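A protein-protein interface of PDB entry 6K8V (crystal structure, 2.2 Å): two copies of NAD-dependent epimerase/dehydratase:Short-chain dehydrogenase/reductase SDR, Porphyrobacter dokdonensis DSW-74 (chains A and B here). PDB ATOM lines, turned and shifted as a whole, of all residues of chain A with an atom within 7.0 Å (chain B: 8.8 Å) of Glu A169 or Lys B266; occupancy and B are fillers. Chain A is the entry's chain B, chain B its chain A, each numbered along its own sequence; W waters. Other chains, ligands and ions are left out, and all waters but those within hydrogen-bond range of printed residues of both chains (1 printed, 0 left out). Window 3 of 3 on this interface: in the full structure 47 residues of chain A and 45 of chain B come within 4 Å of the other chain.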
ATOM      1  N   ASP A 106      14.267  36.374 -23.612  1.00  0.00           N
ATOM      2  CA  ASP A 106      14.752  36.174 -22.219  1.00  0.00           C
ATOM      3  C   ASP A 106      14.375  37.379 -21.356  1.00  0.00           C
ATOM      4  O   ASP A 106      14.071  37.192 -20.166  1.00  0.00           O
ATOM      5  CB  ASP A 106      16.274  36.010 -22.190  1.00  0.00           C
ATOM      6  CG  ASP A 106      16.742  34.672 -22.740  1.00  0.00           C
ATOM      7  OD1 ASP A 106      16.341  33.631 -22.155  1.00  0.00           O
ATOM      8  OD2 ASP A 106      17.476  34.678 -23.759  1.00  0.00           O
ATOM      9  N   ILE A 167       8.845  33.299 -23.703  1.00  0.00           N
ATOM     10  CA  ILE A 167       9.800  33.665 -22.623  1.00  0.00           C
ATOM     11  C   ILE A 167       9.894  32.419 -21.782  1.00  0.00           C
ATOM     12  O   ILE A 167       8.871  31.972 -21.292  1.00  0.00           O
ATOM     13  CB  ILE A 167       9.327  34.844 -21.745  1.00  0.00           C
ATOM     14  CG1 ILE A 167       9.199  36.145 -22.533  1.00  0.00           C
ATOM     15  CG2 ILE A 167      10.233  35.005 -20.538  1.00  0.00           C
ATOM     16  CD1 ILE A 167       8.376  37.205 -21.826  1.00  0.00           C
ATOM     17  N   PRO A 168      11.101  31.861 -21.573  1.00  0.00           N
ATOM     18  CA  PRO A 168      11.256  30.676 -20.752  1.00  0.00           C
ATOM     19  C   PRO A 168      11.229  31.003 -19.255  1.00  0.00           C
ATOM     20  O   PRO A 168      11.288  32.162 -18.867  1.00  0.00           O
ATOM     21  CB  PRO A 168      12.647  30.154 -21.122  1.00  0.00           C
ATOM     22  CG  PRO A 168      13.421  31.400 -21.492  1.00  0.00           C
ATOM     23  CD  PRO A 168      12.394  32.361 -22.065  1.00  0.00           C
ATOM     24  N   GLU A 169      11.183  29.928 -18.472  1.00  0.00           N
ATOM     25  CA  GLU A 169      11.429  29.904 -17.025  1.00  0.00           C
ATOM     26  C   GLU A 169      12.661  30.748 -16.772  1.00  0.00           C
ATOM     27  O   GLU A 169      13.540  30.757 -17.657  1.00  0.00           O
ATOM     28  CB  GLU A 169      11.645  28.458 -16.624  1.00  0.00           C
ATOM     29  CG  GLU A 169      11.232  28.160 -15.209  1.00  0.00           C
ATOM     30  CD  GLU A 169      11.443  26.696 -14.888  1.00  0.00           C
ATOM     31  OE1 GLU A 169      10.739  25.836 -15.502  1.00  0.00           O
ATOM     32  OE2 GLU A 169      12.347  26.425 -14.066  1.00  0.00           O
ATOM     33  N   GLY A 170      12.682  31.468 -15.650  1.00  0.00           N
ATOM     34  CA  GLY A 170      13.775  32.387 -15.279  1.00  0.00           C
ATOM     35  C   GLY A 170      13.855  33.617 -16.171  1.00  0.00           C
ATOM     36  O   GLY A 170      14.833  34.328 -16.050  1.00  0.00           O
ATOM     37  N   GLY A 171      12.856  33.879 -17.025  1.00  0.00           N
ATOM     38  CA  GLY A 171      12.776  35.097 -17.862  1.00  0.00           C
ATOM     39  C   GLY A 171      12.323  36.321 -17.066  1.00  0.00           C
ATOM     40  O   GLY A 171      11.738  36.174 -15.944  1.00  0.00           O
ATOM     41  N   SER A 172      12.540  37.505 -17.634  1.00  0.00           N
ATOM     42  CA  SER A 172      12.374  38.806 -16.932  1.00  0.00           C
ATOM     43  C   SER A 172      11.602  39.776 -17.822  1.00  0.00           C
ATOM     44  O   SER A 172      12.115  40.065 -18.940  1.00  0.00           O
ATOM     45  CB  SER A 172      13.721  39.361 -16.553  1.00  0.00           C
ATOM     46  OG  SER A 172      13.602  40.532 -15.768  1.00  0.00           O
ATOM     47  N   GLY A 210       4.455  34.618 -12.681  1.00  0.00           N
ATOM     48  CA  GLY A 210       5.300  34.124 -11.579  1.00  0.00           C
ATOM     49  C   GLY A 210       5.269  32.598 -11.439  1.00  0.00           C
ATOM     50  O   GLY A 210       6.334  31.975 -11.367  1.00  0.00           O
ATOM     51  N   PRO A 211       4.077  31.948 -11.332  1.00  0.00           N
ATOM     52  CA  PRO A 211       4.016  30.485 -11.208  1.00  0.00           C
ATOM     53  C   PRO A 211       4.694  29.773 -12.392  1.00  0.00           C
ATOM     54  O   PRO A 211       5.253  28.730 -12.185  1.00  0.00           O
ATOM     55  CB  PRO A 211       2.511  30.155 -11.089  1.00  0.00           C
ATOM     56  CG  PRO A 211       1.849  31.473 -10.669  1.00  0.00           C
ATOM     57  CD  PRO A 211       2.739  32.566 -11.240  1.00  0.00           C
ATOM     58  N   LYS A 212       4.713  30.381 -13.573  1.00  0.00           N
ATOM     59  CA  LYS A 212       5.493  29.871 -14.733  1.00  0.00           C
ATOM     60  C   LYS A 212       6.994  30.155 -14.597  1.00  0.00           C
ATOM     61  O   LYS A 212       7.728  29.811 -15.515  1.00  0.00           O
ATOM     62  CB  LYS A 212       5.017  30.529 -16.022  1.00  0.00           C
ATOM     63  CG  LYS A 212       3.539  30.363 -16.329  1.00  0.00           C
ATOM     64  CD  LYS A 212       3.279  30.121 -17.822  1.00  0.00           C
ATOM     65  CE  LYS A 212       2.179  30.982 -18.404  1.00  0.00           C
ATOM     66  NZ  LYS A 212       0.880  30.687 -17.763  1.00  0.00           N
ATOM     67  N   GLY A 213       7.440  30.810 -13.528  1.00  0.00           N
ATOM     68  CA  GLY A 213       8.857  31.180 -13.321  1.00  0.00           C
ATOM     69  C   GLY A 213       9.317  32.413 -14.113  1.00  0.00           C
ATOM     70  O   GLY A 213      10.561  32.589 -14.251  1.00  0.00           O
ATOM     71  N   ILE A 214       8.390  33.244 -14.610  1.00  0.00           N
ATOM     72  CA  ILE A 214       8.703  34.527 -15.319  1.00  0.00           C
ATOM     73  C   ILE A 214       8.487  35.681 -14.336  1.00  0.00           C
ATOM     74  O   ILE A 214       7.406  35.761 -13.781  1.00  0.00           O
ATOM     75  CB  ILE A 214       7.862  34.680 -16.599  1.00  0.00           C
ATOM     76  CG1 ILE A 214       8.174  33.576 -17.614  1.00  0.00           C
ATOM     77  CG2 ILE A 214       8.045  36.064 -17.200  1.00  0.00           C
ATOM     78  CD1 ILE A 214       7.225  33.550 -18.795  1.00  0.00           C
ATOM     79  N   LEU B 257       6.130  34.031  -7.199  1.00  0.00           N
ATOM     80  CA  LEU B 257       7.165  33.501  -8.123  1.00  0.00           C
ATOM     81  C   LEU B 257       7.573  32.069  -7.758  1.00  0.00           C
ATOM     82  O   LEU B 257       7.893  31.804  -6.593  1.00  0.00           O
ATOM     83  CB  LEU B 257       8.397  34.386  -8.077  1.00  0.00           C
ATOM     84  CG  LEU B 257       9.457  33.990  -9.097  1.00  0.00           C
ATOM     85  CD1 LEU B 257       8.984  34.254 -10.513  1.00  0.00           C
ATOM     86  CD2 LEU B 257      10.748  34.707  -8.839  1.00  0.00           C
ATOM     87  N   GLU B 258       7.620  31.202  -8.766  1.00  0.00           N
ATOM     88  CA  GLU B 258       8.152  29.816  -8.694  1.00  0.00           C
ATOM     89  C   GLU B 258       9.528  29.806  -9.359  1.00  0.00           C
ATOM     90  O   GLU B 258       9.716  30.549 -10.337  1.00  0.00           O
ATOM     91  CB  GLU B 258       7.205  28.813  -9.359  1.00  0.00           C
ATOM     92  CG  GLU B 258       5.959  28.536  -8.535  1.00  0.00           C
ATOM     93  CD  GLU B 258       5.172  27.370  -9.074  1.00  0.00           C
ATOM     94  OE1 GLU B 258       5.820  26.471  -9.627  1.00  0.00           O
ATOM     95  OE2 GLU B 258       3.930  27.389  -8.979  1.00  0.00           O
ATOM     96  N   ARG B 259      10.446  28.997  -8.829  1.00  0.00           N
ATOM     97  CA  ARG B 259      11.858  29.016  -9.257  1.00  0.00           C
ATOM     98  C   ARG B 259      12.482  27.628  -9.078  1.00  0.00           C
ATOM     99  O   ARG B 259      12.098  26.914  -8.109  1.00  0.00           O
ATOM    100  CB  ARG B 259      12.587  30.081  -8.441  1.00  0.00           C
ATOM    101  CG  ARG B 259      13.872  30.590  -9.080  1.00  0.00           C
ATOM    102  CD  ARG B 259      14.460  31.594  -8.106  1.00  0.00           C
ATOM    103  NE  ARG B 259      15.893  31.820  -8.202  1.00  0.00           N
ATOM    104  CZ  ARG B 259      16.614  32.390  -7.252  1.00  0.00           C
ATOM    105  NH1 ARG B 259      16.019  32.786  -6.136  1.00  0.00           N
ATOM    106  NH2 ARG B 259      17.921  32.559  -7.411  1.00  0.00           N
ATOM    107  N   ALA B 260      13.432  27.302  -9.963  1.00  0.00           N
ATOM    108  CA  ALA B 260      14.328  26.124  -9.889  1.00  0.00           C
ATOM    109  C   ALA B 260      15.643  26.505  -9.191  1.00  0.00           C
ATOM    110  O   ALA B 260      16.483  27.118  -9.856  1.00  0.00           O
ATOM    111  CB  ALA B 260      14.579  25.613 -11.287  1.00  0.00           C
ATOM    112  N   THR B 261      15.802  26.175  -7.905  1.00  0.00           N
ATOM    113  CA  THR B 261      17.063  26.314  -7.126  1.00  0.00           C
ATOM    114  C   THR B 261      17.552  24.925  -6.697  1.00  0.00           C
ATOM    115  O   THR B 261      16.700  24.009  -6.605  1.00  0.00           O
ATOM    116  CB  THR B 261      16.904  27.233  -5.902  1.00  0.00           C
ATOM    117  OG1 THR B 261      16.077  26.671  -4.874  1.00  0.00           O
ATOM    118  CG2 THR B 261      16.372  28.595  -6.287  1.00  0.00           C
ATOM    119  N   GLY B 263      19.343  22.650  -8.193  1.00  0.00           N
ATOM    120  CA  GLY B 263      19.043  21.650  -9.234  1.00  0.00           C
ATOM    121  C   GLY B 263      17.723  20.903  -9.023  1.00  0.00           C
ATOM    122  O   GLY B 263      17.571  19.865  -9.675  1.00  0.00           O
ATOM    123  N   ASN B 264      16.799  21.369  -8.161  1.00  0.00           N
ATOM    124  CA  ASN B 264      15.419  20.801  -8.017  1.00  0.00           C
ATOM    125  C   ASN B 264      14.639  21.285  -9.236  1.00  0.00           C
ATOM    126  O   ASN B 264      15.217  22.084  -9.983  1.00  0.00           O
ATOM    127  CB  ASN B 264      14.721  21.186  -6.702  1.00  0.00           C
ATOM    128  CG  ASN B 264      15.430  20.667  -5.463  1.00  0.00           C
ATOM    129  OD1 ASN B 264      15.049  20.978  -4.336  1.00  0.00           O
ATOM    130  ND2 ASN B 264      16.458  19.856  -5.645  1.00  0.00           N
ATOM    131  N   GLU B 265      13.393  20.859  -9.420  1.00  0.00           N
ATOM    132  CA  GLU B 265      12.605  21.418 -10.549  1.00  0.00           C
ATOM    133  C   GLU B 265      11.776  22.598 -10.036  1.00  0.00           C
ATOM    134  O   GLU B 265      11.611  22.710  -8.825  1.00  0.00           O
ATOM    135  CB  GLU B 265      11.859  20.361 -11.362  1.00  0.00           C
ATOM    136  CG  GLU B 265      12.630  19.963 -12.613  1.00  0.00           C
ATOM    137  CD  GLU B 265      12.326  18.607 -13.229  1.00  0.00           C
ATOM    138  OE1 GLU B 265      13.078  17.653 -12.946  1.00  0.00           O
ATOM    139  OE2 GLU B 265      11.368  18.518 -14.026  1.00  0.00           O
ATOM    140  N   LYS B 266      11.323  23.447 -10.952  1.00  0.00           N
ATOM    141  CA  LYS B 266      10.545  24.692 -10.667  1.00  0.00           C
ATOM    142  C   LYS B 266       9.493  24.449  -9.584  1.00  0.00           C
ATOM    143  O   LYS B 266       8.748  23.471  -9.722  1.00  0.00           O
ATOM    144  CB  LYS B 266       9.801  25.135 -11.922  1.00  0.00           C
ATOM    145  CG  LYS B 266       9.086  26.470 -11.821  1.00  0.00           C
ATOM    146  CD  LYS B 266       8.186  26.720 -13.007  1.00  0.00           C
ATOM    147  CE  LYS B 266       6.880  25.966 -12.885  1.00  0.00           C
ATOM    148  NZ  LYS B 266       5.993  26.259 -14.030  1.00  0.00           N
ATOM    149  N   ALA B 267       9.431  25.312  -8.566  1.00  0.00           N
ATOM    150  CA  ALA B 267       8.510  25.171  -7.416  1.00  0.00           C
ATOM    151  C   ALA B 267       8.540  26.419  -6.519  1.00  0.00           C
ATOM    152  O   ALA B 267       9.416  27.297  -6.667  1.00  0.00           O
ATOM    153  CB  ALA B 267       8.891  23.954  -6.605  1.00  0.00           C
ATOM    154  N   LYS B 268       7.588  26.477  -5.595  1.00  0.00           N
ATOM    155  CA  LYS B 268       7.608  27.431  -4.471  1.00  0.00           C
ATOM    156  C   LYS B 268       8.753  27.010  -3.559  1.00  0.00           C
ATOM    157  O   LYS B 268       8.610  26.025  -2.844  1.00  0.00           O
ATOM    158  CB  LYS B 268       6.237  27.467  -3.790  1.00  0.00           C
ATOM    159  CG  LYS B 268       5.136  28.064  -4.661  1.00  0.00           C
ATOM    160  CD  LYS B 268       5.332  29.550  -5.047  1.00  0.00           C
ATOM    161  CE  LYS B 268       4.109  30.170  -5.697  1.00  0.00           C
ATOM    162  NZ  LYS B 268       2.989  30.273  -4.725  1.00  0.00           N
ATOM    163  N   THR B 269       9.872  27.716  -3.625  1.00  0.00           N
ATOM    164  CA  THR B 269      11.065  27.434  -2.793  1.00  0.00           C
ATOM    165  C   THR B 269      11.507  28.748  -2.137  1.00  0.00           C
ATOM    166  O   THR B 269      10.798  29.736  -2.256  1.00  0.00           O
ATOM    167  CB  THR B 269      12.149  26.724  -3.618  1.00  0.00           C
ATOM    168  OG1 THR B 269      13.225  26.417  -2.717  1.00  0.00           O
ATOM    169  CG2 THR B 269      12.598  27.569  -4.789  1.00  0.00           C
HETATM  170  O   HOH W   1      13.517  28.890 -12.486  1.00  0.00           O
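No position is printed for both chains.
Of the 9 pairs that touch across the chains among the printed residues, none has its exchanged pair printed and touching as well.
Among the printed residues, pairs that only touch across the chains: Gly A213 with Glu B258, Glu A169 with Lys B266, Gly A210 with Leu B257, Glu A169 with Ala B260, Lys A212 with Lys B266 and Ile A214 with Leu B257.
N of Gly A170 lies within hydrogen-bond range of O of Gly A213, at 2.8 Å.
Water W1 bridges N of Ala B260 and OE2 of Glu A169.
Ile A167 touches none of the printed residues of chain B.
Of chain B, only Ala B260 and Lys B266 come within 4 Å of Glu A169.
Printed residues of chain B within 4 Å of Gly A210: Leu B257 (3.6 Å) and Glu B258 (3.0 Å).
Of the printed residues of chain B, Gly A213 touches Glu B258.
Of the printed residues of chain A, Glu B258 touches Gly A210 (3.0 Å), Pro A211 (3.4 Å) and Gly A213 (3.2 Å).
Of chain A, only Glu A169 (3.6 Å), Pro A211 (3.2 Å) and Lys A212 (3.7 Å) come within 4 Å of Lys B266.
Lys B268 touches none of the printed residues of chain A.
The nearest residue of chain B that does not touch Glu A169 is Arg B259 (5.1 Å).
The nearest printed residue of chain A that does not touch Glu B258 is Lys A212 (5.1 Å).
The backbone carbonyl oxygen (O) of Gly A210 sits at hydrogen-bond distance from the backbone NH (N) of Glu B258 (3.0 Å).
O of Pro A211 is in hydrogen-bond range of NZ of Lys B266 (3.2 Å).
OE1 of Glu B258 lies close to O of Pro A211, at 3.5 Å.
Hydrophobic or aromatic side chains of chain A that line the printed part of chain B: Pro A211.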
